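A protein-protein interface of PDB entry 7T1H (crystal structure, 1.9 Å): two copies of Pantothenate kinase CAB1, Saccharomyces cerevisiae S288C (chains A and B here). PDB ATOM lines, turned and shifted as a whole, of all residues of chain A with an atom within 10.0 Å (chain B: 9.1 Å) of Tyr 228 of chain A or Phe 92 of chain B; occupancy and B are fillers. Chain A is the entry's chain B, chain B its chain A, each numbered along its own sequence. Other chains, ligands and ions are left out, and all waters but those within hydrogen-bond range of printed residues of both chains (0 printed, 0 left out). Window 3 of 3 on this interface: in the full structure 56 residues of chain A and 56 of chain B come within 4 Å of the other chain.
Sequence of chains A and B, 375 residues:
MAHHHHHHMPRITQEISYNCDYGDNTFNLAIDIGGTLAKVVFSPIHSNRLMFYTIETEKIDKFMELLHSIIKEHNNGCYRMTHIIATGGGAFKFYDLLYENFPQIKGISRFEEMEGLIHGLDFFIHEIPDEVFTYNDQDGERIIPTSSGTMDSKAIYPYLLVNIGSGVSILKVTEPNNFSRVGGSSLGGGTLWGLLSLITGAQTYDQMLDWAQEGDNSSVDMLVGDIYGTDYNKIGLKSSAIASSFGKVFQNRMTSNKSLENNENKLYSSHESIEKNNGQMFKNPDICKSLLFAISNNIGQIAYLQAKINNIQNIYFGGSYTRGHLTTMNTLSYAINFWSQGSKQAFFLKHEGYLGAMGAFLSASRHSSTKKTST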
ATOM      1  N   MET A 222     -25.678  -8.457  23.332  1.00  0.00           N
ATOM      2  CA  MET A 222     -24.434  -8.047  22.628  1.00  0.00           C
ATOM      3  C   MET A 222     -23.427  -9.166  22.842  1.00  0.00           C
ATOM      4  O   MET A 222     -23.117  -9.466  24.035  1.00  0.00           O
ATOM      5  CB  MET A 222     -23.817  -6.746  23.145  1.00  0.00           C
ATOM      6  CG  MET A 222     -24.677  -5.534  22.964  1.00  0.00           C
ATOM      7  SD  MET A 222     -23.808  -4.012  23.519  1.00  0.00           S
ATOM      8  CE  MET A 222     -22.756  -3.693  22.108  1.00  0.00           C
ATOM      9  N   LEU A 223     -23.007  -9.821  21.762  1.00  0.00           N
ATOM     10  CA  LEU A 223     -21.958 -10.865  21.804  1.00  0.00           C
ATOM     11  C   LEU A 223     -20.608 -10.207  21.528  1.00  0.00           C
ATOM     12  O   LEU A 223     -20.574  -9.075  21.048  1.00  0.00           O
ATOM     13  CB  LEU A 223     -22.266 -11.951  20.768  1.00  0.00           C
ATOM     14  CG  LEU A 223     -23.665 -12.556  20.867  1.00  0.00           C
ATOM     15  CD1 LEU A 223     -23.831 -13.726  19.898  1.00  0.00           C
ATOM     16  CD2 LEU A 223     -23.948 -12.993  22.279  1.00  0.00           C
ATOM     17  N   VAL A 224     -19.542 -10.888  21.896  1.00  0.00           N
ATOM     18  CA  VAL A 224     -18.142 -10.421  21.697  1.00  0.00           C
ATOM     19  C   VAL A 224     -17.991  -9.978  20.234  1.00  0.00           C
ATOM     20  O   VAL A 224     -17.556  -8.842  20.018  1.00  0.00           O
ATOM     21  CB  VAL A 224     -17.164 -11.533  22.133  1.00  0.00           C
ATOM     22  CG1 VAL A 224     -15.738 -11.308  21.646  1.00  0.00           C
ATOM     23  CG2 VAL A 224     -17.182 -11.693  23.648  1.00  0.00           C
ATOM     24  N   GLY A 225     -18.448 -10.804  19.283  1.00  0.00           N
ATOM     25  CA  GLY A 225     -18.447 -10.528  17.832  1.00  0.00           C
ATOM     26  C   GLY A 225     -19.139  -9.221  17.478  1.00  0.00           C
ATOM     27  O   GLY A 225     -18.650  -8.528  16.574  1.00  0.00           O
ATOM     28  N   ASP A 226     -20.252  -8.900  18.137  1.00  0.00           N
ATOM     29  CA  ASP A 226     -21.048  -7.671  17.891  1.00  0.00           C
ATOM     30  C   ASP A 226     -20.248  -6.419  18.281  1.00  0.00           C
ATOM     31  O   ASP A 226     -20.437  -5.363  17.617  1.00  0.00           O
ATOM     32  CB  ASP A 226     -22.369  -7.695  18.667  1.00  0.00           C
ATOM     33  CG  ASP A 226     -23.299  -8.854  18.330  1.00  0.00           C
ATOM     34  OD1 ASP A 226     -23.240  -9.368  17.175  1.00  0.00           O
ATOM     35  OD2 ASP A 226     -24.080  -9.250  19.224  1.00  0.00           O
ATOM     36  N   ILE A 227     -19.453  -6.482  19.356  1.00  0.00           N
ATOM     37  CA  ILE A 227     -18.645  -5.316  19.822  1.00  0.00           C
ATOM     38  C   ILE A 227     -17.368  -5.220  18.972  1.00  0.00           C
ATOM     39  O   ILE A 227     -17.022  -4.095  18.605  1.00  0.00           O
ATOM     40  CB  ILE A 227     -18.313  -5.385  21.327  1.00  0.00           C
ATOM     41  CG1 ILE A 227     -19.547  -5.686  22.185  1.00  0.00           C
ATOM     42  CG2 ILE A 227     -17.638  -4.099  21.770  1.00  0.00           C
ATOM     43  CD1 ILE A 227     -19.366  -5.419  23.672  1.00  0.00           C
ATOM     44  N   TYR A 228     -16.686  -6.347  18.711  1.00  0.00           N
ATOM     45  CA  TYR A 228     -15.321  -6.405  18.113  1.00  0.00           C
ATOM     46  C   TYR A 228     -15.383  -6.659  16.600  1.00  0.00           C
ATOM     47  O   TYR A 228     -14.956  -5.739  15.843  1.00  0.00           O
ATOM     48  CB  TYR A 228     -14.466  -7.477  18.793  1.00  0.00           C
ATOM     49  CG  TYR A 228     -14.189  -7.194  20.246  1.00  0.00           C
ATOM     50  CD1 TYR A 228     -13.167  -6.341  20.621  1.00  0.00           C
ATOM     51  CD2 TYR A 228     -14.961  -7.755  21.248  1.00  0.00           C
ATOM     52  CE1 TYR A 228     -12.916  -6.058  21.952  1.00  0.00           C
ATOM     53  CE2 TYR A 228     -14.735  -7.468  22.585  1.00  0.00           C
ATOM     54  CZ  TYR A 228     -13.709  -6.611  22.939  1.00  0.00           C
ATOM     55  OH  TYR A 228     -13.452  -6.327  24.249  1.00  0.00           O
ATOM     56  N   GLY A 229     -15.845  -7.857  16.197  1.00  0.00           N
ATOM     57  CA  GLY A 229     -15.867  -8.363  14.808  1.00  0.00           C
ATOM     58  C   GLY A 229     -14.664  -9.256  14.524  1.00  0.00           C
ATOM     59  O   GLY A 229     -14.296  -9.381  13.319  1.00  0.00           O
ATOM     60  N   LYS A 238     -14.179 -16.049  22.186  1.00  0.00           N
ATOM     61  CA  LYS A 238     -15.176 -16.861  21.432  1.00  0.00           C
ATOM     62  C   LYS A 238     -16.259 -15.907  20.947  1.00  0.00           C
ATOM     63  O   LYS A 238     -16.691 -15.067  21.753  1.00  0.00           O
ATOM     64  CB  LYS A 238     -15.764 -17.976  22.299  1.00  0.00           C
ATOM     65  CG  LYS A 238     -16.552 -19.040  21.543  1.00  0.00           C
ATOM     66  CD  LYS A 238     -17.023 -20.194  22.425  1.00  0.00           C
ATOM     67  CE  LYS A 238     -17.386 -21.448  21.653  1.00  0.00           C
ATOM     68  NZ  LYS A 238     -18.458 -21.188  20.665  1.00  0.00           N
ATOM     69  N   SER A 239     -16.633 -15.994  19.672  1.00  0.00           N
ATOM     70  CA  SER A 239     -17.495 -14.992  18.990  1.00  0.00           C
ATOM     71  C   SER A 239     -18.870 -14.944  19.675  1.00  0.00           C
ATOM     72  O   SER A 239     -19.388 -13.817  19.856  1.00  0.00           O
ATOM     73  CB  SER A 239     -17.600 -15.270  17.503  1.00  0.00           C
ATOM     74  OG  SER A 239     -17.657 -14.052  16.767  1.00  0.00           O
ATOM     75  N   SER A 240     -19.377 -16.116  20.089  1.00  0.00           N
ATOM     76  CA  SER A 240     -20.719 -16.365  20.687  1.00  0.00           C
ATOM     77  C   SER A 240     -20.771 -16.063  22.201  1.00  0.00           C
ATOM     78  O   SER A 240     -21.890 -16.143  22.779  1.00  0.00           O
ATOM     79  CB  SER A 240     -21.147 -17.792  20.414  1.00  0.00           C
ATOM     80  OG  SER A 240     -20.594 -18.701  21.365  1.00  0.00           O
ATOM     81  N   ALA A 241     -19.638 -15.772  22.844  1.00  0.00           N
ATOM     82  CA  ALA A 241     -19.562 -15.285  24.243  1.00  0.00           C
ATOM     83  C   ALA A 241     -20.412 -14.014  24.400  1.00  0.00           C
ATOM     84  O   ALA A 241     -20.416 -13.154  23.488  1.00  0.00           O
ATOM     85  CB  ALA A 241     -18.130 -15.023  24.647  1.00  0.00           C
ATOM     86  N   ILE A 242     -21.116 -13.898  25.523  1.00  0.00           N
ATOM     87  CA  ILE A 242     -22.045 -12.762  25.775  1.00  0.00           C
ATOM     88  C   ILE A 242     -21.253 -11.643  26.438  1.00  0.00           C
ATOM     89  O   ILE A 242     -20.814 -11.845  27.536  1.00  0.00           O
ATOM     90  CB  ILE A 242     -23.233 -13.216  26.628  1.00  0.00           C
ATOM     91  CG1 ILE A 242     -23.991 -14.359  25.948  1.00  0.00           C
ATOM     92  CG2 ILE A 242     -24.139 -12.026  26.918  1.00  0.00           C
ATOM     93  CD1 ILE A 242     -24.753 -15.245  26.875  1.00  0.00           C
ATOM     94  N   ALA A 243     -21.128 -10.495  25.790  1.00  0.00           N
ATOM     95  CA  ALA A 243     -20.522  -9.276  26.360  1.00  0.00           C
ATOM     96  C   ALA A 243     -21.551  -8.533  27.229  1.00  0.00           C
ATOM     97  O   ALA A 243     -21.190  -8.049  28.303  1.00  0.00           O
ATOM     98  CB  ALA A 243     -20.001  -8.402  25.253  1.00  0.00           C
ATOM     99  N   SER A 244     -22.806  -8.454  26.811  1.00  0.00           N
ATOM    100  CA  SER A 244     -23.861  -7.721  27.566  1.00  0.00           C
ATOM    101  C   SER A 244     -25.196  -8.434  27.387  1.00  0.00           C
ATOM    102  O   SER A 244     -25.751  -8.361  26.282  1.00  0.00           O
ATOM    103  CB  SER A 244     -23.944  -6.280  27.153  1.00  0.00           C
ATOM    104  OG  SER A 244     -24.965  -5.598  27.881  1.00  0.00           O
ATOM    105  N   ILE B  31     -10.570   8.663  20.805  1.00  0.00           N
ATOM    106  CA  ILE B  31     -11.973   8.174  20.875  1.00  0.00           C
ATOM    107  C   ILE B  31     -12.042   6.770  21.480  1.00  0.00           C
ATOM    108  O   ILE B  31     -11.441   5.836  20.908  1.00  0.00           O
ATOM    109  CB  ILE B  31     -12.624   8.208  19.494  1.00  0.00           C
ATOM    110  CG1 ILE B  31     -12.306   9.516  18.767  1.00  0.00           C
ATOM    111  CG2 ILE B  31     -14.113   7.995  19.667  1.00  0.00           C
ATOM    112  CD1 ILE B  31     -12.780   9.512  17.360  1.00  0.00           C
ATOM    113  N   ILE B  33     -14.524   3.917  21.720  1.00  0.00           N
ATOM    114  CA  ILE B  33     -15.816   3.483  21.122  1.00  0.00           C
ATOM    115  C   ILE B  33     -16.265   2.218  21.843  1.00  0.00           C
ATOM    116  O   ILE B  33     -15.617   1.172  21.673  1.00  0.00           O
ATOM    117  CB  ILE B  33     -15.736   3.299  19.601  1.00  0.00           C
ATOM    118  CG1 ILE B  33     -15.143   4.535  18.923  1.00  0.00           C
ATOM    119  CG2 ILE B  33     -17.111   2.939  19.059  1.00  0.00           C
ATOM    120  CD1 ILE B  33     -15.260   4.541  17.408  1.00  0.00           C
ATOM    121  N   GLY B  34     -17.350   2.318  22.607  1.00  0.00           N
ATOM    122  CA  GLY B  34     -17.852   1.168  23.385  1.00  0.00           C
ATOM    123  C   GLY B  34     -18.978   0.445  22.672  1.00  0.00           C
ATOM    124  O   GLY B  34     -19.063   0.515  21.414  1.00  0.00           O
ATOM    125  N   GLY B  35     -19.828  -0.230  23.449  1.00  0.00           N
ATOM    126  CA  GLY B  35     -21.057  -0.843  22.927  1.00  0.00           C
ATOM    127  C   GLY B  35     -22.024   0.196  22.388  1.00  0.00           C
ATOM    128  O   GLY B  35     -22.486   0.003  21.249  1.00  0.00           O
ATOM    129  N   ALA B  86      -8.109   5.515  18.138  1.00  0.00           N
ATOM    130  CA  ALA B  86      -9.360   4.838  18.529  1.00  0.00           C
ATOM    131  C   ALA B  86      -9.042   3.725  19.528  1.00  0.00           C
ATOM    132  O   ALA B  86      -8.006   3.028  19.372  1.00  0.00           O
ATOM    133  CB  ALA B  86     -10.094   4.337  17.308  1.00  0.00           C
ATOM    134  N   THR B  87      -9.891   3.582  20.545  1.00  0.00           N
ATOM    135  CA  THR B  87      -9.756   2.522  21.583  1.00  0.00           C
ATOM    136  C   THR B  87     -11.168   2.052  21.920  1.00  0.00           C
ATOM    137  O   THR B  87     -12.103   2.549  21.303  1.00  0.00           O
ATOM    138  CB  THR B  87      -8.912   2.995  22.781  1.00  0.00           C
ATOM    139  OG1 THR B  87      -8.522   1.815  23.477  1.00  0.00           O
ATOM    140  CG2 THR B  87      -9.638   3.929  23.723  1.00  0.00           C
ATOM    141  N   GLY B  88     -11.284   1.115  22.852  1.00  0.00           N
ATOM    142  CA  GLY B  88     -12.519   0.381  23.140  1.00  0.00           C
ATOM    143  C   GLY B  88     -12.698  -0.794  22.205  1.00  0.00           C
ATOM    144  O   GLY B  88     -12.155  -0.769  21.092  1.00  0.00           O
ATOM    145  N   GLY B  89     -13.529  -1.750  22.603  1.00  0.00           N
ATOM    146  CA  GLY B  89     -13.871  -2.908  21.763  1.00  0.00           C
ATOM    147  C   GLY B  89     -14.238  -2.494  20.350  1.00  0.00           C
ATOM    148  O   GLY B  89     -13.936  -3.275  19.438  1.00  0.00           O
ATOM    149  N   GLY B  90     -14.849  -1.313  20.178  1.00  0.00           N
ATOM    150  CA  GLY B  90     -15.369  -0.784  18.897  1.00  0.00           C
ATOM    151  C   GLY B  90     -14.306  -0.183  17.985  1.00  0.00           C
ATOM    152  O   GLY B  90     -14.674   0.217  16.868  1.00  0.00           O
ATOM    153  N   ALA B  91     -13.045  -0.097  18.421  1.00  0.00           N
ATOM    154  CA  ALA B  91     -11.925   0.505  17.646  1.00  0.00           C
ATOM    155  C   ALA B  91     -11.758  -0.253  16.320  1.00  0.00           C
ATOM    156  O   ALA B  91     -11.452   0.386  15.298  1.00  0.00           O
ATOM    157  CB  ALA B  91     -10.646   0.484  18.453  1.00  0.00           C
ATOM    158  N   PHE B  92     -12.002  -1.569  16.330  1.00  0.00           N
ATOM    159  CA  PHE B  92     -11.849  -2.462  15.154  1.00  0.00           C
ATOM    160  C   PHE B  92     -13.044  -2.254  14.220  1.00  0.00           C
ATOM    161  O   PHE B  92     -12.842  -1.993  13.044  1.00  0.00           O
ATOM    162  CB  PHE B  92     -11.689  -3.914  15.620  1.00  0.00           C
ATOM    163  N   LYS B  93     -14.259  -2.301  14.759  1.00  0.00           N
ATOM    164  CA  LYS B  93     -15.518  -2.304  13.981  1.00  0.00           C
ATOM    165  C   LYS B  93     -15.699  -0.981  13.230  1.00  0.00           C
ATOM    166  O   LYS B  93     -16.270  -1.048  12.141  1.00  0.00           O
ATOM    167  CB  LYS B  93     -16.705  -2.561  14.914  1.00  0.00           C
ATOM    168  CG  LYS B  93     -18.051  -2.801  14.239  1.00  0.00           C
ATOM    169  CD  LYS B  93     -19.173  -3.151  15.221  1.00  0.00           C
ATOM    170  CE  LYS B  93     -20.566  -2.869  14.682  1.00  0.00           C
ATOM    171  NZ  LYS B  93     -21.625  -3.110  15.697  1.00  0.00           N
ATOM    172  N   PHE B  94     -15.286   0.173  13.788  1.00  0.00           N
ATOM    173  CA  PHE B  94     -15.522   1.508  13.164  1.00  0.00           C
ATOM    174  C   PHE B  94     -14.246   2.105  12.542  1.00  0.00           C
ATOM    175  O   PHE B  94     -14.299   3.253  12.064  1.00  0.00           O
ATOM    176  CB  PHE B  94     -16.210   2.448  14.161  1.00  0.00           C
ATOM    177  CG  PHE B  94     -17.609   2.003  14.515  1.00  0.00           C
ATOM    178  CD1 PHE B  94     -18.442   1.421  13.565  1.00  0.00           C
ATOM    179  CD2 PHE B  94     -18.095   2.147  15.800  1.00  0.00           C
ATOM    180  CE1 PHE B  94     -19.723   1.000  13.897  1.00  0.00           C
ATOM    181  CE2 PHE B  94     -19.373   1.727  16.135  1.00  0.00           C
ATOM    182  CZ  PHE B  94     -20.186   1.154  15.182  1.00  0.00           C
ATOM    183  N   TYR B  95     -13.164   1.338  12.420  1.00  0.00           N
ATOM    184  CA  TYR B  95     -11.888   1.847  11.843  1.00  0.00           C
ATOM    185  C   TYR B  95     -12.165   2.359  10.420  1.00  0.00           C
ATOM    186  O   TYR B  95     -11.724   3.476  10.084  1.00  0.00           O
ATOM    187  CB  TYR B  95     -10.779   0.791  11.906  1.00  0.00           C
ATOM    188  CG  TYR B  95      -9.393   1.306  11.585  1.00  0.00           C
ATOM    189  CD1 TYR B  95      -8.624   1.954  12.542  1.00  0.00           C
ATOM    190  CD2 TYR B  95      -8.828   1.122  10.329  1.00  0.00           C
ATOM    191  CE1 TYR B  95      -7.343   2.412  12.263  1.00  0.00           C
ATOM    192  CE2 TYR B  95      -7.554   1.588  10.027  1.00  0.00           C
ATOM    193  CZ  TYR B  95      -6.807   2.239  10.997  1.00  0.00           C
ATOM    194  OH  TYR B  95      -5.545   2.694  10.712  1.00  0.00           O
ATOM    195  N   ASP B  96     -12.910   1.572   9.635  1.00  0.00           N
ATOM    196  CA  ASP B  96     -13.235   1.844   8.209  1.00  0.00           C
ATOM    197  C   ASP B  96     -14.192   3.034   8.119  1.00  0.00           C
ATOM    198  O   ASP B  96     -13.982   3.873   7.260  1.00  0.00           O
ATOM    199  CB  ASP B  96     -13.788   0.595   7.520  1.00  0.00           C
ATOM    200  CG  ASP B  96     -12.708  -0.415   7.153  1.00  0.00           C
ATOM    201  OD1 ASP B  96     -11.505  -0.126   7.411  1.00  0.00           O
ATOM    202  OD2 ASP B  96     -13.073  -1.501   6.636  1.00  0.00           O
ATOM    203  N   LEU B  97     -15.197   3.110   8.984  1.00  0.00           N
ATOM    204  CA  LEU B  97     -16.079   4.302   9.056  1.00  0.00           C
ATOM    205  C   LEU B  97     -15.165   5.515   9.272  1.00  0.00           C
ATOM    206  O   LEU B  97     -15.328   6.509   8.549  1.00  0.00           O
ATOM    207  CB  LEU B  97     -17.116   4.125  10.173  1.00  0.00           C
ATOM    208  CG  LEU B  97     -18.503   4.738   9.967  1.00  0.00           C
ATOM    209  CD1 LEU B  97     -19.053   4.455   8.576  1.00  0.00           C
ATOM    210  CD2 LEU B  97     -19.473   4.203  11.016  1.00  0.00           C
ATOM    211  N   LEU B  98     -14.191   5.436  10.186  1.00  0.00           N
ATOM    212  CA  LEU B  98     -13.330   6.608  10.476  1.00  0.00           C
ATOM    213  C   LEU B  98     -12.489   6.951   9.240  1.00  0.00           C
ATOM    214  O   LEU B  98     -12.371   8.128   8.948  1.00  0.00           O
ATOM    215  CB  LEU B  98     -12.449   6.353  11.698  1.00  0.00           C
ATOM    216  CG  LEU B  98     -13.196   6.334  13.031  1.00  0.00           C
ATOM    217  CD1 LEU B  98     -12.284   5.860  14.154  1.00  0.00           C
ATOM    218  CD2 LEU B  98     -13.749   7.709  13.344  1.00  0.00           C
ATOM    219  N   SER B 109      -4.767   5.680  14.272  1.00  0.00           N
ATOM    220  CA  SER B 109      -4.188   4.485  14.928  1.00  0.00           C
ATOM    221  C   SER B 109      -5.204   3.899  15.925  1.00  0.00           C
ATOM    222  O   SER B 109      -6.287   4.520  16.177  1.00  0.00           O
ATOM    223  CB  SER B 109      -2.890   4.814  15.604  1.00  0.00           C
ATOM    224  OG  SER B 109      -3.056   5.831  16.586  1.00  0.00           O
ATOM    225  N   ARG B 110      -4.857   2.740  16.473  1.00  0.00           N
ATOM    226  CA  ARG B 110      -5.668   2.015  17.475  1.00  0.00           C
ATOM    227  C   ARG B 110      -4.820   1.902  18.728  1.00  0.00           C
ATOM    228  O   ARG B 110      -3.586   1.768  18.586  1.00  0.00           O
ATOM    229  CB  ARG B 110      -5.989   0.580  17.054  1.00  0.00           C
ATOM    230  CG  ARG B 110      -7.059   0.418  15.987  1.00  0.00           C
ATOM    231  CD  ARG B 110      -7.401  -1.064  15.840  1.00  0.00           C
ATOM    232  NE  ARG B 110      -7.673  -1.382  14.448  1.00  0.00           N
ATOM    233  CZ  ARG B 110      -6.745  -1.442  13.493  1.00  0.00           C
ATOM    234  NH1 ARG B 110      -5.470  -1.225  13.780  1.00  0.00           N
ATOM    235  NH2 ARG B 110      -7.103  -1.700  12.244  1.00  0.00           N
ATOM    236  N   PHE B 111      -5.461   1.899  19.894  1.00  0.00           N
ATOM    237  CA  PHE B 111      -4.802   1.587  21.180  1.00  0.00           C
ATOM    238  C   PHE B 111      -5.602   0.500  21.895  1.00  0.00           C
ATOM    239  O   PHE B 111      -6.832   0.624  22.043  1.00  0.00           O
ATOM    240  CB  PHE B 111      -4.719   2.836  22.047  1.00  0.00           C
ATOM    241  CG  PHE B 111      -3.648   2.787  23.099  1.00  0.00           C
ATOM    242  CD1 PHE B 111      -2.322   2.613  22.746  1.00  0.00           C
ATOM    243  CD2 PHE B 111      -3.963   2.957  24.440  1.00  0.00           C
ATOM    244  CE1 PHE B 111      -1.325   2.611  23.712  1.00  0.00           C
ATOM    245  CE2 PHE B 111      -2.968   2.955  25.404  1.00  0.00           C
ATOM    246  CZ  PHE B 111      -1.647   2.775  25.036  1.00  0.00           C
ATOM    247  N   GLU B 112      -4.880  -0.481  22.413  1.00  0.00           N
ATOM    248  CA  GLU B 112      -5.449  -1.674  23.084  1.00  0.00           C
ATOM    249  C   GLU B 112      -6.330  -1.207  24.256  1.00  0.00           C
ATOM    250  O   GLU B 112      -5.953  -0.240  24.957  1.00  0.00           O
ATOM    251  CB  GLU B 112      -4.302  -2.609  23.466  1.00  0.00           C
ATOM    252  CG  GLU B 112      -4.784  -3.992  23.844  1.00  0.00           C
ATOM    253  CD  GLU B 112      -5.188  -4.115  25.299  1.00  0.00           C
ATOM    254  OE1 GLU B 112      -4.433  -3.587  26.165  1.00  0.00           O
ATOM    255  OE2 GLU B 112      -6.265  -4.705  25.565  1.00  0.00           O
ATOM    256  N   GLU B 113      -7.486  -1.827  24.405  1.00  0.00           N
ATOM    257  CA  GLU B 113      -8.559  -1.411  25.341  1.00  0.00           C
ATOM    258  C   GLU B 113      -8.049  -1.396  26.796  1.00  0.00           C
ATOM    259  O   GLU B 113      -8.223  -0.373  27.506  1.00  0.00           O
ATOM    260  CB  GLU B 113      -9.724  -2.369  25.130  1.00  0.00           C
ATOM    261  CG  GLU B 113     -10.917  -2.086  25.999  1.00  0.00           C
ATOM    262  CD  GLU B 113     -12.104  -2.979  25.678  1.00  0.00           C
ATOM    263  OE1 GLU B 113     -11.898  -3.983  24.935  1.00  0.00           O
ATOM    264  OE2 GLU B 113     -13.226  -2.660  26.164  1.00  0.00           O
ATOM    265  N   MET B 114      -7.424  -2.477  27.268  1.00  0.00           N
ATOM    266  CA  MET B 114      -7.081  -2.592  28.715  1.00  0.00           C
ATOM    267  C   MET B 114      -5.946  -1.600  29.051  1.00  0.00           C
ATOM    268  O   MET B 114      -6.057  -0.818  30.027  1.00  0.00           O
ATOM    269  CB  MET B 114      -6.730  -4.044  29.062  1.00  0.00           C
ATOM    270  CG  MET B 114      -7.823  -5.059  28.653  1.00  0.00           C
ATOM    271  SD  MET B 114      -9.603  -4.733  29.153  1.00  0.00           S
ATOM    272  CE  MET B 114     -10.495  -5.752  27.976  1.00  0.00           C
ATOM    273  N   LEU B 117      -7.401   1.844  29.283  1.00  0.00           N
ATOM    274  CA  LEU B 117      -8.138   2.023  30.563  1.00  0.00           C
ATOM    275  C   LEU B 117      -7.130   2.274  31.681  1.00  0.00           C
ATOM    276  O   LEU B 117      -7.348   3.219  32.459  1.00  0.00           O
ATOM    277  CB  LEU B 117      -8.985   0.789  30.882  1.00  0.00           C
ATOM    278  CG  LEU B 117     -10.225   0.648  30.010  1.00  0.00           C
ATOM    279  CD1 LEU B 117     -10.817  -0.721  30.155  1.00  0.00           C
ATOM    280  CD2 LEU B 117     -11.236   1.741  30.322  1.00  0.00           C
ATOM    281  N   SER B 169     -16.049  -5.123  32.703  1.00  0.00           N
ATOM    282  CA  SER B 169     -14.645  -5.585  32.613  1.00  0.00           C
ATOM    283  C   SER B 169     -13.984  -5.303  33.955  1.00  0.00           C
ATOM    284  O   SER B 169     -14.250  -4.228  34.529  1.00  0.00           O
ATOM    285  CB  SER B 169     -13.887  -4.878  31.507  1.00  0.00           C
ATOM    286  OG  SER B 169     -14.509  -5.170  30.281  1.00  0.00           O
ATOM    287  N   ARG B 181      -6.375  -8.560  33.024  1.00  0.00           N
ATOM    288  CA  ARG B 181      -7.828  -8.771  33.051  1.00  0.00           C
ATOM    289  C   ARG B 181      -8.111  -9.940  33.992  1.00  0.00           C
ATOM    290  O   ARG B 181      -7.305 -10.875  34.025  1.00  0.00           O
ATOM    291  CB  ARG B 181      -8.318  -9.030  31.630  1.00  0.00           C
ATOM    292  CG  ARG B 181      -9.818  -8.875  31.477  1.00  0.00           C
ATOM    293  CD  ARG B 181     -10.212  -9.037  30.024  1.00  0.00           C
ATOM    294  NE  ARG B 181     -11.378  -8.245  29.658  1.00  0.00           N
ATOM    295  CZ  ARG B 181     -12.608  -8.720  29.475  1.00  0.00           C
ATOM    296  NH1 ARG B 181     -12.871 -10.012  29.642  1.00  0.00           N
ATOM    297  NH2 ARG B 181     -13.578  -7.893  29.118  1.00  0.00           N
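NZ of Lys 93 of chain B sits at hydrogen-bond distance from O of Asp 226 of chain A (3.2 Å).
The side-chain hydroxyl (OH) of Tyr 228 of chain A is in hydrogen-bond range of the side-chain carboxylate (OE1) of Glu 113 of chain B.
O of Ile 227 of chain A sits close to O of Gly 89 of chain B, at 3.3 Å.
Hydrophobic or aromatic side chains of chain B within 4 Å of the printed part of chain A: Phe 92.
Hydrophobic or aromatic side chains of chain A that line the printed part of chain B: Met 222, Ile 227 and Tyr 228.
Among the printed residues, no Asp or Glu carboxylate lies within 4 Å of a Lys or Arg side-chain nitrogen of the other chain.
Of the printed residues of chain B, Met 222 of chain A touches Gly 35 (3.4 Å).
Of the printed residues of chain B, Ile 227 of chain A touches Gly 89 and Gly 90.
No residue of chain B comes within 4 Å of Gly 229 of chain A.
Ala 243 of chain A touches none of the printed residues of chain B.
Gly 89 of chain B touches just these residues of chain A: Ile 227 and Tyr 228.
No residue of chain A comes within 4 Å of Ala 91 of chain B.
Of chain A, only Tyr 228 (3.7 Å) comes within 4 Å of Phe 92 of chain B.
Of the printed residues of chain A, Lys 93 of chain B touches Asp 226 and Tyr 228.
Of the printed residues of chain A, Glu 113 of chain B touches Tyr 228 (2.9 Å).
The backbone carbonyl oxygen (O) of Ile 33 of chain B sits at hydrogen-bond distance from the backbone NH (N) of Gly 90 of chain B (3.0 Å).
The backbone carbonyl oxygen (O) of Met 222 of chain A is in hydrogen-bond range of the backbone NH (N) of Ala 243 of chain A (2.8 Å).
The backbone carbonyl oxygen of Ser 244 of chain A lies within hydrogen-bond range of the backbone NH of Met 222 of chain A (3.0 Å).
The side-chain carboxylate of Asp 226 of chain A is in hydrogen-bond range of the backbone NH of Leu 223 of chain A, at 2.8 Å.
No position is printed for both chains.
Of the 8 pairs that touch across the chains among the printed residues, none has its exchanged pair printed and touching as well.
Among the printed residues, pairs that only touch across the chains: Met 222 of chain A with Gly 35 of chain B (3.4 Å), Ile 227 of chain A with Gly 90 of chain B (3.7 Å), Tyr 228 of chain A with Gly 89 of chain B (3.3 Å), Tyr 228 of chain A with Phe 92 of chain B (3.7 Å) and Tyr 228 of chain A with Lys 93 of chain B (3.7 Å).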
